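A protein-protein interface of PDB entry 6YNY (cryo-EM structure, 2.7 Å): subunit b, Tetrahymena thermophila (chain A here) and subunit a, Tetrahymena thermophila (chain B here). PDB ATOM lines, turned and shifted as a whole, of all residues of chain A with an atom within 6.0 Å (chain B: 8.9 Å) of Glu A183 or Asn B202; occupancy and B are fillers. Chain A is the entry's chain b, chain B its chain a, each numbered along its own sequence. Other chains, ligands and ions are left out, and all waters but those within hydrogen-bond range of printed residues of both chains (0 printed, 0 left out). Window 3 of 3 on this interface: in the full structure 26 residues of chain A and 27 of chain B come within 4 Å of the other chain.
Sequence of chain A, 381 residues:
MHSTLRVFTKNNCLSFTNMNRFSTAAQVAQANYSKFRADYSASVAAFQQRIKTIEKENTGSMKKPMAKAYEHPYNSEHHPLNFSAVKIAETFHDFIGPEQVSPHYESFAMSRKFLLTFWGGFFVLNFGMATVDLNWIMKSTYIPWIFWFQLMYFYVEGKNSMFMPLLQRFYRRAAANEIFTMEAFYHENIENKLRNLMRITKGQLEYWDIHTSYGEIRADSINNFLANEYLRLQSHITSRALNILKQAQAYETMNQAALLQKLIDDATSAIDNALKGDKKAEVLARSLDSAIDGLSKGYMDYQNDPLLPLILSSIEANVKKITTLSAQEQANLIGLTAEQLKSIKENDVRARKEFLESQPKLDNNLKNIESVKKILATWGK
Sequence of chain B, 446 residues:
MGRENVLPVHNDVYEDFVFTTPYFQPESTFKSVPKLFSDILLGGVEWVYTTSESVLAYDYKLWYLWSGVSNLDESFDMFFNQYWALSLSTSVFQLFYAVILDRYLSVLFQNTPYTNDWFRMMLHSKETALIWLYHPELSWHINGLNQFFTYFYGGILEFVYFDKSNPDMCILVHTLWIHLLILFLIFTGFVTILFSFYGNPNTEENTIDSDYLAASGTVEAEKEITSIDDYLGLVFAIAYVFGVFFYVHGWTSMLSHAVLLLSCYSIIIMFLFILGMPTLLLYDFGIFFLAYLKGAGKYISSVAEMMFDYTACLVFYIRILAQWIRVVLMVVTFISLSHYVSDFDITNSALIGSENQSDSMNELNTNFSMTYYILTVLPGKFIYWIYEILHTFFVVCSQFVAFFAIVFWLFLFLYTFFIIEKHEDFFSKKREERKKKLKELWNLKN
Of chain B, only Asn B202 comes within 4 Å of Glu A183.
No residue of chain B comes within 4 Å of Ala A184.
Of the printed residues of chain B, Phe A180 touches Thr B203 (3.5 Å).
Of the printed residues of chain A, Ile B208 touches Ala A176 (3.5 Å).
Printed residues of chain A within 4 Å of Thr B203: Phe A180.
Printed residues of chain B within 4 Å of Ala A176: Asn B202, Ile B208 and Tyr B212.
Gly B199 touches none of the printed residues of chain A.
Pro B201 touches none of the printed residues of chain A.
The nearest residue of chain B that does not touch Glu A183 is Asn B200 (6.7 Å).
The nearest residue of chain A that does not touch Asn B202 is Phe A180 (4.1 Å).
Among the printed residues, pairs that only touch across the chains: Ile A179 with Asn B202 (3.4 Å), Ala A176 with Ile B208 (3.5 Å), Ile A179 with Tyr B212 (3.5 Å), Phe A180 with Thr B203 (3.5 Å), Ala A176 with Asn B202 (3.7 Å), Ala A176 with Tyr B212 (3.7 Å) and Glu A183 with Asn B202 (3.9 Å).
Hydrophobic or aromatic side chains of chain A that line the printed part of chain B: Ala A176, Ile A179 and Phe A180.
Of the 13 printed residues of chain B, 4 touch a printed residue of chain A.
Hydrophobic or aromatic side chains of chain B within 4 Å of the printed part of chain A: Ile B208 and Tyr B212.
N of Asn B202 lies within hydrogen-bond range of OD1 of Asn B200, 2.8 Å away.
The side-chain amide nitrogen (ND2) of Asn B200 sits close to the side-chain hydroxyl (OG1) of Thr B203 (3.4 Å).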
ATOM      1  N   ALA A 176      16.482 -14.088 -14.288  1.00  0.00           N
ATOM      2  CA  ALA A 176      15.265 -13.714 -13.581  1.00  0.00           C
ATOM      3  C   ALA A 176      14.156 -14.732 -13.809  1.00  0.00           C
ATOM      4  O   ALA A 176      13.387 -15.035 -12.891  1.00  0.00           O
ATOM      5  CB  ALA A 176      14.812 -12.328 -14.031  1.00  0.00           C
ATOM      6  N   ASN A 177      14.058 -15.266 -15.026  1.00  0.00           N
ATOM      7  CA  ASN A 177      13.016 -16.238 -15.326  1.00  0.00           C
ATOM      8  C   ASN A 177      13.225 -17.538 -14.567  1.00  0.00           C
ATOM      9  O   ASN A 177      12.252 -18.187 -14.171  1.00  0.00           O
ATOM     10  CB  ASN A 177      12.974 -16.499 -16.829  1.00  0.00           C
ATOM     11  CG  ASN A 177      11.733 -17.243 -17.257  1.00  0.00           C
ATOM     12  OD1 ASN A 177      10.658 -16.659 -17.371  1.00  0.00           O
ATOM     13  ND2 ASN A 177      11.875 -18.533 -17.510  1.00  0.00           N
ATOM     14  N   GLU A 178      14.479 -17.934 -14.355  1.00  0.00           N
ATOM     15  CA  GLU A 178      14.750 -19.135 -13.578  1.00  0.00           C
ATOM     16  C   GLU A 178      14.471 -18.905 -12.101  1.00  0.00           C
ATOM     17  O   GLU A 178      13.947 -19.790 -11.417  1.00  0.00           O
ATOM     18  CB  GLU A 178      16.194 -19.579 -13.794  1.00  0.00           C
ATOM     19  CG  GLU A 178      16.578 -20.835 -13.045  1.00  0.00           C
ATOM     20  CD  GLU A 178      17.886 -21.424 -13.528  1.00  0.00           C
ATOM     21  OE1 GLU A 178      18.703 -20.675 -14.105  1.00  0.00           O
ATOM     22  OE2 GLU A 178      18.097 -22.639 -13.339  1.00  0.00           O
ATOM     23  N   ILE A 179      14.802 -17.718 -11.595  1.00  0.00           N
ATOM     24  CA  ILE A 179      14.501 -17.391 -10.207  1.00  0.00           C
ATOM     25  C   ILE A 179      12.998 -17.284  -9.995  1.00  0.00           C
ATOM     26  O   ILE A 179      12.467 -17.747  -8.981  1.00  0.00           O
ATOM     27  CB  ILE A 179      15.220 -16.093  -9.806  1.00  0.00           C
ATOM     28  CG1 ILE A 179      16.730 -16.309  -9.815  1.00  0.00           C
ATOM     29  CG2 ILE A 179      14.746 -15.625  -8.454  1.00  0.00           C
ATOM     30  CD1 ILE A 179      17.522 -15.061  -9.678  1.00  0.00           C
ATOM     31  N   PHE A 180      12.292 -16.666 -10.941  1.00  0.00           N
ATOM     32  CA  PHE A 180      10.839 -16.602 -10.849  1.00  0.00           C
ATOM     33  C   PHE A 180      10.238 -17.995 -10.762  1.00  0.00           C
ATOM     34  O   PHE A 180       9.260 -18.216 -10.038  1.00  0.00           O
ATOM     35  CB  PHE A 180      10.275 -15.854 -12.054  1.00  0.00           C
ATOM     36  CG  PHE A 180       8.783 -15.927 -12.173  1.00  0.00           C
ATOM     37  CD1 PHE A 180       7.980 -14.983 -11.569  1.00  0.00           C
ATOM     38  CD2 PHE A 180       8.182 -16.939 -12.896  1.00  0.00           C
ATOM     39  CE1 PHE A 180       6.615 -15.051 -11.680  1.00  0.00           C
ATOM     40  CE2 PHE A 180       6.818 -17.005 -13.003  1.00  0.00           C
ATOM     41  CZ  PHE A 180       6.036 -16.062 -12.397  1.00  0.00           C
ATOM     42  N   THR A 181      10.817 -18.950 -11.487  1.00  0.00           N
ATOM     43  CA  THR A 181      10.304 -20.311 -11.464  1.00  0.00           C
ATOM     44  C   THR A 181      10.628 -21.002 -10.145  1.00  0.00           C
ATOM     45  O   THR A 181       9.816 -21.777  -9.631  1.00  0.00           O
ATOM     46  CB  THR A 181      10.879 -21.091 -12.644  1.00  0.00           C
ATOM     47  OG1 THR A 181      10.695 -20.342 -13.850  1.00  0.00           O
ATOM     48  CG2 THR A 181      10.192 -22.415 -12.791  1.00  0.00           C
ATOM     49  N   MET A 182      11.802 -20.727  -9.576  1.00  0.00           N
ATOM     50  CA  MET A 182      12.136 -21.297  -8.275  1.00  0.00           C
ATOM     51  C   MET A 182      11.213 -20.769  -7.187  1.00  0.00           C
ATOM     52  O   MET A 182      10.782 -21.527  -6.312  1.00  0.00           O
ATOM     53  CB  MET A 182      13.590 -21.000  -7.928  1.00  0.00           C
ATOM     54  CG  MET A 182      14.588 -21.690  -8.824  1.00  0.00           C
ATOM     55  SD  MET A 182      16.295 -21.351  -8.375  1.00  0.00           S
ATOM     56  CE  MET A 182      16.356 -22.153  -6.779  1.00  0.00           C
ATOM     57  N   GLU A 183      10.906 -19.471  -7.215  1.00  0.00           N
ATOM     58  CA  GLU A 183       9.951 -18.922  -6.261  1.00  0.00           C
ATOM     59  C   GLU A 183       8.590 -19.586  -6.403  1.00  0.00           C
ATOM     60  O   GLU A 183       7.880 -19.771  -5.410  1.00  0.00           O
ATOM     61  CB  GLU A 183       9.827 -17.413  -6.456  1.00  0.00           C
ATOM     62  CG  GLU A 183      11.119 -16.640  -6.258  1.00  0.00           C
ATOM     63  CD  GLU A 183      11.556 -16.567  -4.809  1.00  0.00           C
ATOM     64  OE1 GLU A 183      11.024 -17.332  -3.980  1.00  0.00           O
ATOM     65  OE2 GLU A 183      12.435 -15.736  -4.497  1.00  0.00           O
ATOM     66  N   ALA A 184       8.212 -19.951  -7.628  1.00  0.00           N
ATOM     67  CA  ALA A 184       6.946 -20.635  -7.845  1.00  0.00           C
ATOM     68  C   ALA A 184       6.930 -22.012  -7.198  1.00  0.00           C
ATOM     69  O   ALA A 184       5.861 -22.504  -6.822  1.00  0.00           O
ATOM     70  CB  ALA A 184       6.670 -20.750  -9.340  1.00  0.00           C
ATOM     71  N   PHE A 185       8.091 -22.649  -7.068  1.00  0.00           N
ATOM     72  CA  PHE A 185       8.209 -23.956  -6.437  1.00  0.00           C
ATOM     73  C   PHE A 185       8.896 -23.876  -5.078  1.00  0.00           C
ATOM     74  O   PHE A 185       9.565 -24.822  -4.661  1.00  0.00           O
ATOM     75  CB  PHE A 185       8.961 -24.924  -7.346  1.00  0.00           C
ATOM     76  CG  PHE A 185       8.241 -25.247  -8.617  1.00  0.00           C
ATOM     77  CD1 PHE A 185       7.289 -26.242  -8.652  1.00  0.00           C
ATOM     78  CD2 PHE A 185       8.524 -24.565  -9.781  1.00  0.00           C
ATOM     79  CE1 PHE A 185       6.630 -26.541  -9.818  1.00  0.00           C
ATOM     80  CE2 PHE A 185       7.869 -24.861 -10.945  1.00  0.00           C
ATOM     81  CZ  PHE A 185       6.921 -25.848 -10.964  1.00  0.00           C
ATOM     82  N   TYR A 186       8.745 -22.751  -4.378  1.00  0.00           N
ATOM     83  CA  TYR A 186       9.347 -22.628  -3.055  1.00  0.00           C
ATOM     84  C   TYR A 186       8.748 -23.631  -2.081  1.00  0.00           C
ATOM     85  O   TYR A 186       9.468 -24.236  -1.279  1.00  0.00           O
ATOM     86  CB  TYR A 186       9.174 -21.208  -2.524  1.00  0.00           C
ATOM     87  CG  TYR A 186       9.567 -21.058  -1.075  1.00  0.00           C
ATOM     88  CD1 TYR A 186      10.895 -20.953  -0.704  1.00  0.00           C
ATOM     89  CD2 TYR A 186       8.608 -21.025  -0.079  1.00  0.00           C
ATOM     90  CE1 TYR A 186      11.255 -20.820   0.614  1.00  0.00           C
ATOM     91  CE2 TYR A 186       8.961 -20.891   1.240  1.00  0.00           C
ATOM     92  CZ  TYR A 186      10.285 -20.791   1.582  1.00  0.00           C
ATOM     93  OH  TYR A 186      10.634 -20.658   2.901  1.00  0.00           O
ATOM     94  N   HIS A 187       7.430 -23.821  -2.136  1.00  0.00           N
ATOM     95  CA  HIS A 187       6.775 -24.742  -1.216  1.00  0.00           C
ATOM     96  C   HIS A 187       7.233 -26.173  -1.452  1.00  0.00           C
ATOM     97  O   HIS A 187       7.456 -26.928  -0.498  1.00  0.00           O
ATOM     98  CB  HIS A 187       5.259 -24.640  -1.367  1.00  0.00           C
ATOM     99  CG  HIS A 187       4.711 -23.277  -1.096  1.00  0.00           C
ATOM    100  ND1 HIS A 187       5.024 -22.181  -1.870  1.00  0.00           N
ATOM    101  CD2 HIS A 187       3.858 -22.833  -0.144  1.00  0.00           C
ATOM    102  CE1 HIS A 187       4.395 -21.119  -1.400  1.00  0.00           C
ATOM    103  NE2 HIS A 187       3.681 -21.488  -0.353  1.00  0.00           N
ATOM    104  N   GLY B 199       8.624  -4.211  -5.456  1.00  0.00           N
ATOM    105  CA  GLY B 199       7.624  -5.081  -6.030  1.00  0.00           C
ATOM    106  C   GLY B 199       8.189  -6.462  -6.272  1.00  0.00           C
ATOM    107  O   GLY B 199       8.865  -7.016  -5.402  1.00  0.00           O
ATOM    108  N   ASN B 200       7.926  -7.032  -7.446  1.00  0.00           N
ATOM    109  CA  ASN B 200       8.509  -8.315  -7.808  1.00  0.00           C
ATOM    110  C   ASN B 200       9.821  -8.066  -8.536  1.00  0.00           C
ATOM    111  O   ASN B 200       9.796  -7.604  -9.686  1.00  0.00           O
ATOM    112  CB  ASN B 200       7.563  -9.117  -8.680  1.00  0.00           C
ATOM    113  CG  ASN B 200       8.051 -10.533  -8.911  1.00  0.00           C
ATOM    114  OD1 ASN B 200       9.248 -10.804  -8.874  1.00  0.00           O
ATOM    115  ND2 ASN B 200       7.123 -11.444  -9.145  1.00  0.00           N
ATOM    116  N   PRO B 201      10.975  -8.353  -7.931  1.00  0.00           N
ATOM    117  CA  PRO B 201      12.248  -8.107  -8.615  1.00  0.00           C
ATOM    118  C   PRO B 201      12.546  -9.094  -9.727  1.00  0.00           C
ATOM    119  O   PRO B 201      13.546  -8.922 -10.433  1.00  0.00           O
ATOM    120  CB  PRO B 201      13.270  -8.236  -7.481  1.00  0.00           C
ATOM    121  CG  PRO B 201      12.658  -9.212  -6.567  1.00  0.00           C
ATOM    122  CD  PRO B 201      11.182  -8.971  -6.613  1.00  0.00           C
ATOM    123  N   ASN B 202      11.708 -10.109  -9.909  1.00  0.00           N
ATOM    124  CA  ASN B 202      11.942 -11.162 -10.881  1.00  0.00           C
ATOM    125  C   ASN B 202      11.078 -11.027 -12.125  1.00  0.00           C
ATOM    126  O   ASN B 202      11.325 -11.731 -13.110  1.00  0.00           O
ATOM    127  CB  ASN B 202      11.695 -12.522 -10.226  1.00  0.00           C
ATOM    128  CG  ASN B 202      12.482 -12.699  -8.946  1.00  0.00           C
ATOM    129  OD1 ASN B 202      13.670 -12.395  -8.891  1.00  0.00           O
ATOM    130  ND2 ASN B 202      11.819 -13.182  -7.904  1.00  0.00           N
ATOM    131  N   THR B 203      10.081 -10.144 -12.108  1.00  0.00           N
ATOM    132  CA  THR B 203       9.242  -9.890 -13.268  1.00  0.00           C
ATOM    133  C   THR B 203       9.337  -8.466 -13.789  1.00  0.00           C
ATOM    134  O   THR B 203       9.035  -8.241 -14.965  1.00  0.00           O
ATOM    135  CB  THR B 203       7.770 -10.188 -12.951  1.00  0.00           C
ATOM    136  OG1 THR B 203       7.342  -9.387 -11.845  1.00  0.00           O
ATOM    137  CG2 THR B 203       7.581 -11.649 -12.620  1.00  0.00           C
ATOM    138  N   GLU B 204       9.742  -7.509 -12.962  1.00  0.00           N
ATOM    139  CA  GLU B 204       9.862  -6.116 -13.370  1.00  0.00           C
ATOM    140  C   GLU B 204      11.255  -5.902 -13.944  1.00  0.00           C
ATOM    141  O   GLU B 204      12.243  -5.869 -13.204  1.00  0.00           O
ATOM    142  CB  GLU B 204       9.590  -5.191 -12.188  1.00  0.00           C
ATOM    143  CG  GLU B 204       8.181  -5.315 -11.643  1.00  0.00           C
ATOM    144  CD  GLU B 204       7.948  -4.473 -10.409  1.00  0.00           C
ATOM    145  OE1 GLU B 204       8.868  -3.728 -10.011  1.00  0.00           O
ATOM    146  OE2 GLU B 204       6.843  -4.558  -9.836  1.00  0.00           O
ATOM    147  N   GLU B 205      11.336  -5.756 -15.265  1.00  0.00           N
ATOM    148  CA  GLU B 205      12.629  -5.654 -15.926  1.00  0.00           C
ATOM    149  C   GLU B 205      13.387  -4.391 -15.544  1.00  0.00           C
ATOM    150  O   GLU B 205      14.602  -4.331 -15.747  1.00  0.00           O
ATOM    151  CB  GLU B 205      12.442  -5.708 -17.440  1.00  0.00           C
ATOM    152  CG  GLU B 205      12.093  -7.086 -17.958  1.00  0.00           C
ATOM    153  CD  GLU B 205      11.945  -7.130 -19.466  1.00  0.00           C
ATOM    154  OE1 GLU B 205      10.965  -7.732 -19.950  1.00  0.00           O
ATOM    155  OE2 GLU B 205      12.804  -6.558 -20.167  1.00  0.00           O
ATOM    156  N   ASN B 206      12.707  -3.389 -14.988  1.00  0.00           N
ATOM    157  CA  ASN B 206      13.394  -2.157 -14.625  1.00  0.00           C
ATOM    158  C   ASN B 206      14.334  -2.376 -13.447  1.00  0.00           C
ATOM    159  O   ASN B 206      15.449  -1.845 -13.431  1.00  0.00           O
ATOM    160  CB  ASN B 206      12.377  -1.063 -14.310  1.00  0.00           C
ATOM    161  CG  ASN B 206      13.025   0.285 -14.103  1.00  0.00           C
ATOM    162  OD1 ASN B 206      13.459   0.929 -15.055  1.00  0.00           O
ATOM    163  ND2 ASN B 206      13.089   0.723 -12.858  1.00  0.00           N
ATOM    164  N   THR B 207      13.901  -3.148 -12.452  1.00  0.00           N
ATOM    165  CA  THR B 207      14.775  -3.479 -11.334  1.00  0.00           C
ATOM    166  C   THR B 207      15.712  -4.633 -11.667  1.00  0.00           C
ATOM    167  O   THR B 207      16.819  -4.699 -11.124  1.00  0.00           O
ATOM    168  CB  THR B 207      13.942  -3.813 -10.094  1.00  0.00           C
ATOM    169  OG1 THR B 207      14.805  -4.081  -8.986  1.00  0.00           O
ATOM    170  CG2 THR B 207      13.095  -5.011 -10.332  1.00  0.00           C
ATOM    171  N   ILE B 208      15.295  -5.542 -12.547  1.00  0.00           N
ATOM    172  CA  ILE B 208      16.202  -6.580 -13.024  1.00  0.00           C
ATOM    173  C   ILE B 208      17.427  -5.952 -13.670  1.00  0.00           C
ATOM    174  O   ILE B 208      18.570  -6.306 -13.360  1.00  0.00           O
ATOM    175  CB  ILE B 208      15.475  -7.518 -14.005  1.00  0.00           C
ATOM    176  CG1 ILE B 208      14.411  -8.341 -13.279  1.00  0.00           C
ATOM    177  CG2 ILE B 208      16.470  -8.408 -14.721  1.00  0.00           C
ATOM    178  CD1 ILE B 208      13.482  -9.088 -14.199  1.00  0.00           C
ATOM    179  N   ASP B 209      17.205  -5.002 -14.578  1.00  0.00           N
ATOM    180  CA  ASP B 209      18.319  -4.374 -15.275  1.00  0.00           C
ATOM    181  C   ASP B 209      19.222  -3.618 -14.310  1.00  0.00           C
ATOM    182  O   ASP B 209      20.449  -3.636 -14.455  1.00  0.00           O
ATOM    183  CB  ASP B 209      17.792  -3.443 -16.364  1.00  0.00           C
ATOM    184  CG  ASP B 209      17.154  -4.193 -17.511  1.00  0.00           C
ATOM    185  OD1 ASP B 209      17.606  -5.318 -17.808  1.00  0.00           O
ATOM    186  OD2 ASP B 209      16.207  -3.656 -18.120  1.00  0.00           O
ATOM    187  N   ASP B 211      19.428  -4.044 -10.854  1.00  0.00           N
ATOM    188  CA  ASP B 211      20.015  -4.898  -9.830  1.00  0.00           C
ATOM    189  C   ASP B 211      21.215  -5.664 -10.371  1.00  0.00           C
ATOM    190  O   ASP B 211      22.288  -5.672  -9.756  1.00  0.00           O
ATOM    191  CB  ASP B 211      18.962  -5.864  -9.293  1.00  0.00           C
ATOM    192  CG  ASP B 211      19.484  -6.729  -8.169  1.00  0.00           C
ATOM    193  OD1 ASP B 211      20.625  -6.504  -7.719  1.00  0.00           O
ATOM    194  OD2 ASP B 211      18.752  -7.639  -7.736  1.00  0.00           O
ATOM    195  N   TYR B 212      21.053  -6.319 -11.518  1.00  0.00           N
ATOM    196  CA  TYR B 212      22.150  -7.091 -12.090  1.00  0.00           C
ATOM    197  C   TYR B 212      23.277  -6.185 -12.568  1.00  0.00           C
ATOM    198  O   TYR B 212      24.455  -6.544 -12.461  1.00  0.00           O
ATOM    199  CB  TYR B 212      21.629  -7.955 -13.235  1.00  0.00           C
ATOM    200  CG  TYR B 212      20.753  -9.106 -12.799  1.00  0.00           C
ATOM    201  CD1 TYR B 212      21.171 -10.417 -12.948  1.00  0.00           C
ATOM    202  CD2 TYR B 212      19.508  -8.881 -12.243  1.00  0.00           C
ATOM    203  CE1 TYR B 212      20.375 -11.464 -12.552  1.00  0.00           C
ATOM    204  CE2 TYR B 212      18.708  -9.921 -11.847  1.00  0.00           C
ATOM    205  CZ  TYR B 212      19.144 -11.210 -12.002  1.00  0.00           C
ATOM    206  OH  TYR B 212      18.339 -12.245 -11.605  1.00  0.00           O
